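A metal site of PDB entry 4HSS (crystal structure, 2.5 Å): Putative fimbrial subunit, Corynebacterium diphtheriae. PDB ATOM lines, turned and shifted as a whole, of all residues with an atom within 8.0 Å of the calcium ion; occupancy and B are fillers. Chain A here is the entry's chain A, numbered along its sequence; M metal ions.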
ATOM      1  N   LYS A 303     -23.500   2.683 -19.040  1.00  0.00           N
ATOM      2  CA  LYS A 303     -22.536   1.618 -19.262  1.00  0.00           C
ATOM      3  C   LYS A 303     -22.446   1.275 -20.744  1.00  0.00           C
ATOM      4  O   LYS A 303     -23.435   1.368 -21.477  1.00  0.00           O
ATOM      5  CB  LYS A 303     -22.943   0.377 -18.440  1.00  0.00           C
ATOM      6  CG  LYS A 303     -22.832   0.601 -16.929  1.00  0.00           C
ATOM      7  CD  LYS A 303     -23.013  -0.717 -16.144  1.00  0.00           C
ATOM      8  CE  LYS A 303     -24.370  -0.836 -15.526  1.00  0.00           C
ATOM      9  NZ  LYS A 303     -24.457  -1.993 -14.589  1.00  0.00           N
ATOM     10  N   THR A 402     -25.867   8.815 -26.056  1.00  0.00           N
ATOM     11  CA  THR A 402     -26.821   9.814 -25.591  1.00  0.00           C
ATOM     12  C   THR A 402     -27.761   9.183 -24.625  1.00  0.00           C
ATOM     13  O   THR A 402     -27.954   7.970 -24.690  1.00  0.00           O
ATOM     14  CB  THR A 402     -27.605  10.416 -26.760  1.00  0.00           C
ATOM     15  OG1 THR A 402     -28.423   9.392 -27.334  1.00  0.00           O
ATOM     16  CG2 THR A 402     -26.704  11.087 -27.793  1.00  0.00           C
ATOM     17  N   ARG A 403     -28.365   9.997 -23.731  1.00  0.00           N
ATOM     18  CA  ARG A 403     -29.316   9.553 -22.727  1.00  0.00           C
ATOM     19  C   ARG A 403     -30.408   8.695 -23.334  1.00  0.00           C
ATOM     20  O   ARG A 403     -30.711   7.641 -22.782  1.00  0.00           O
ATOM     21  CB  ARG A 403     -29.960  10.757 -22.043  1.00  0.00           C
ATOM     22  CG  ARG A 403     -29.043  11.583 -21.179  1.00  0.00           C
ATOM     23  CD  ARG A 403     -29.835  12.678 -20.531  1.00  0.00           C
ATOM     24  NE  ARG A 403     -30.268  13.682 -21.502  1.00  0.00           N
ATOM     25  CZ  ARG A 403     -31.032  14.723 -21.220  1.00  0.00           C
ATOM     26  NH1 ARG A 403     -31.477  14.908 -19.980  1.00  0.00           N
ATOM     27  NH2 ARG A 403     -31.360  15.588 -22.159  1.00  0.00           N
ATOM     28  N   ALA A 404     -30.971   9.148 -24.455  1.00  0.00           N
ATOM     29  CA  ALA A 404     -32.055   8.483 -25.195  1.00  0.00           C
ATOM     30  C   ALA A 404     -31.629   7.119 -25.728  1.00  0.00           C
ATOM     31  O   ALA A 404     -32.336   6.138 -25.510  1.00  0.00           O
ATOM     32  CB  ALA A 404     -32.534   9.376 -26.360  1.00  0.00           C
ATOM     33  N   LYS A 405     -30.480   7.044 -26.409  1.00  0.00           N
ATOM     34  CA  LYS A 405     -29.941   5.794 -26.959  1.00  0.00           C
ATOM     35  C   LYS A 405     -29.544   4.795 -25.865  1.00  0.00           C
ATOM     36  O   LYS A 405     -29.678   3.607 -26.102  1.00  0.00           O
ATOM     37  CB  LYS A 405     -28.747   6.046 -27.892  1.00  0.00           C
ATOM     38  CG  LYS A 405     -29.128   6.566 -29.280  1.00  0.00           C
ATOM     39  CD  LYS A 405     -29.259   5.448 -30.302  1.00  0.00           C
ATOM     40  CE  LYS A 405     -29.296   5.944 -31.725  1.00  0.00           C
ATOM     41  NZ  LYS A 405     -29.064   4.815 -32.693  1.00  0.00           N
ATOM     42  N   ILE A 406     -29.083   5.233 -24.690  1.00  0.00           N
ATOM     43  CA  ILE A 406     -28.701   4.336 -23.585  1.00  0.00           C
ATOM     44  C   ILE A 406     -29.974   3.821 -22.931  1.00  0.00           C
ATOM     45  O   ILE A 406     -29.965   2.755 -22.336  1.00  0.00           O
ATOM     46  CB  ILE A 406     -27.759   5.068 -22.559  1.00  0.00           C
ATOM     47  CG1 ILE A 406     -26.428   5.479 -23.190  1.00  0.00           C
ATOM     48  CG2 ILE A 406     -27.486   4.271 -21.275  1.00  0.00           C
ATOM     49  CD1 ILE A 406     -25.814   6.671 -22.546  1.00  0.00           C
ATOM     50  N   SER A 407     -31.051   4.599 -22.975  1.00  0.00           N
ATOM     51  CA  SER A 407     -32.353   4.290 -22.362  1.00  0.00           C
ATOM     52  C   SER A 407     -33.137   3.214 -23.145  1.00  0.00           C
ATOM     53  O   SER A 407     -34.052   2.632 -22.568  1.00  0.00           O
ATOM     54  CB  SER A 407     -33.201   5.549 -22.275  1.00  0.00           C
ATOM     55  OG  SER A 407     -34.403   5.279 -21.574  1.00  0.00           O
ATOM     56  N   GLU A 408     -32.802   2.966 -24.405  1.00  0.00           N
ATOM     57  CA  GLU A 408     -33.504   1.956 -25.210  1.00  0.00           C
ATOM     58  C   GLU A 408     -33.362   0.547 -24.567  1.00  0.00           C
ATOM     59  O   GLU A 408     -32.331   0.255 -23.951  1.00  0.00           O
ATOM     60  CB  GLU A 408     -33.003   1.945 -26.676  1.00  0.00           C
ATOM     61  CG  GLU A 408     -33.232   3.247 -27.431  1.00  0.00           C
ATOM     62  CD  GLU A 408     -32.930   3.233 -28.914  1.00  0.00           C
ATOM     63  OE1 GLU A 408     -33.350   2.272 -29.598  1.00  0.00           O
ATOM     64  OE2 GLU A 408     -32.329   4.217 -29.405  1.00  0.00           O
ATOM     65  N   LYS A 409     -34.406  -0.256 -24.602  1.00  0.00           N
ATOM     66  CA  LYS A 409     -34.317  -1.595 -24.006  1.00  0.00           C
ATOM     67  C   LYS A 409     -34.314  -2.637 -25.108  1.00  0.00           C
ATOM     68  O   LYS A 409     -34.867  -2.414 -26.185  1.00  0.00           O
ATOM     69  CB  LYS A 409     -35.433  -1.835 -22.997  1.00  0.00           C
ATOM     70  CG  LYS A 409     -35.368  -0.884 -21.786  1.00  0.00           C
ATOM     71  CD  LYS A 409     -36.312  -1.291 -20.676  1.00  0.00           C
ATOM     72  CE  LYS A 409     -35.718  -2.330 -19.736  1.00  0.00           C
ATOM     73  NZ  LYS A 409     -34.788  -1.731 -18.749  1.00  0.00           N
ATOM     74  N   ASP A 410     -33.622  -3.742 -24.895  1.00  0.00           N
ATOM     75  CA  ASP A 410     -33.547  -4.864 -25.827  1.00  0.00           C
ATOM     76  C   ASP A 410     -33.347  -6.105 -24.969  1.00  0.00           C
ATOM     77  O   ASP A 410     -32.222  -6.442 -24.608  1.00  0.00           O
ATOM     78  CB  ASP A 410     -32.415  -4.661 -26.885  1.00  0.00           C
ATOM     79  CG  ASP A 410     -32.239  -5.720 -27.977  1.00  0.00           C
ATOM     80  OD1 ASP A 410     -33.180  -6.537 -28.192  1.00  0.00           O
ATOM     81  OD2 ASP A 410     -31.198  -5.688 -28.663  1.00  0.00           O
ATOM     82  N   ASP A 416     -30.409  -3.097 -21.139  1.00  0.00           N
ATOM     83  CA  ASP A 416     -31.306  -2.443 -20.186  1.00  0.00           C
ATOM     84  C   ASP A 416     -31.181  -0.887 -20.282  1.00  0.00           C
ATOM     85  O   ASP A 416     -30.417  -0.371 -21.117  1.00  0.00           O
ATOM     86  CB  ASP A 416     -31.102  -2.961 -18.731  1.00  0.00           C
ATOM     87  CG  ASP A 416     -29.738  -2.696 -18.045  1.00  0.00           C
ATOM     88  OD1 ASP A 416     -28.956  -1.858 -18.558  1.00  0.00           O
ATOM     89  OD2 ASP A 416     -29.473  -3.321 -16.988  1.00  0.00           O
ATOM     90  N   GLU A 417     -31.963  -0.162 -19.416  1.00  0.00           N
ATOM     91  CA  GLU A 417     -32.092   1.300 -19.331  1.00  0.00           C
ATOM     92  C   GLU A 417     -30.773   2.048 -19.039  1.00  0.00           C
ATOM     93  O   GLU A 417     -30.730   3.259 -19.272  1.00  0.00           O
ATOM     94  CB  GLU A 417     -33.147   1.703 -18.244  1.00  0.00           C
ATOM     95  CG  GLU A 417     -32.758   1.324 -16.812  1.00  0.00           C
ATOM     96  CD  GLU A 417     -33.669   1.792 -15.684  1.00  0.00           C
ATOM     97  OE1 GLU A 417     -33.436   2.896 -15.133  1.00  0.00           O
ATOM     98  OE2 GLU A 417     -34.530   0.982 -15.268  1.00  0.00           O
ATOM     99  N   VAL A 418     -29.726   1.368 -18.445  1.00  0.00           N
ATOM    100  CA  VAL A 418     -28.500   2.091 -18.064  1.00  0.00           C
ATOM    101  C   VAL A 418     -27.300   1.656 -18.904  1.00  0.00           C
ATOM    102  O   VAL A 418     -26.227   2.256 -18.774  1.00  0.00           O
ATOM    103  CB  VAL A 418     -28.174   2.042 -16.535  1.00  0.00           C
ATOM    104  CG1 VAL A 418     -29.356   2.521 -15.710  1.00  0.00           C
ATOM    105  CG2 VAL A 418     -27.709   0.657 -16.073  1.00  0.00           C
ATOM    106  N   THR A 419     -27.495   0.689 -19.812  1.00  0.00           N
ATOM    107  CA  THR A 419     -26.462   0.103 -20.674  1.00  0.00           C
ATOM    108  C   THR A 419     -26.785   0.263 -22.156  1.00  0.00           C
ATOM    109  O   THR A 419     -27.910  -0.022 -22.567  1.00  0.00           O
ATOM    110  CB  THR A 419     -26.319  -1.415 -20.353  1.00  0.00           C
ATOM    111  OG1 THR A 419     -26.239  -1.587 -18.943  1.00  0.00           O
ATOM    112  CG2 THR A 419     -25.125  -2.065 -21.026  1.00  0.00           C
ATOM    113  N   LEU A 420     -25.774   0.676 -22.955  1.00  0.00           N
ATOM    114  CA  LEU A 420     -25.816   0.737 -24.403  1.00  0.00           C
ATOM    115  C   LEU A 420     -24.908  -0.437 -24.908  1.00  0.00           C
ATOM    116  O   LEU A 420     -23.744  -0.507 -24.515  1.00  0.00           O
ATOM    117  CB  LEU A 420     -25.376   2.115 -24.923  1.00  0.00           C
ATOM    118  CG  LEU A 420     -25.471   2.394 -26.446  1.00  0.00           C
ATOM    119  CD1 LEU A 420     -25.543   3.895 -26.713  1.00  0.00           C
ATOM    120  CD2 LEU A 420     -24.283   1.895 -27.158  1.00  0.00           C
ATOM    121  N   VAL A 421     -25.465  -1.348 -25.723  1.00  0.00           N
ATOM    122  CA  VAL A 421     -24.767  -2.533 -26.242  1.00  0.00           C
ATOM    123  C   VAL A 421     -24.318  -2.316 -27.699  1.00  0.00           C
ATOM    124  O   VAL A 421     -25.144  -1.970 -28.549  1.00  0.00           O
ATOM    125  CB  VAL A 421     -25.606  -3.820 -26.079  1.00  0.00           C
ATOM    126  CG1 VAL A 421     -24.940  -5.016 -26.740  1.00  0.00           C
ATOM    127  CG2 VAL A 421     -25.876  -4.126 -24.614  1.00  0.00           C
HETATM  128 CA    CA M   1     -30.018   0.363 -23.591  1.00  0.00          CA
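The calcium ion is bound by the backbone carbonyl oxygen of Glu 408, the backbone carbonyl oxygen of Thr 419, the backbone carbonyl oxygen of Asp 416 and the backbone carbonyl oxygen of Ile 406.
The calcium ion has four donor atoms within binding distance.
The backbone NH (N) of Val 418 lies close to the side-chain carboxylate (OD1) of Asp 416, 3.3 Å away.
OG1 of Thr 419 is in hydrogen-bond range of OD1 of Asp 416, 2.8 Å away.
Of the 16 residues printed, 4 come within 4 Å of the calcium ion.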
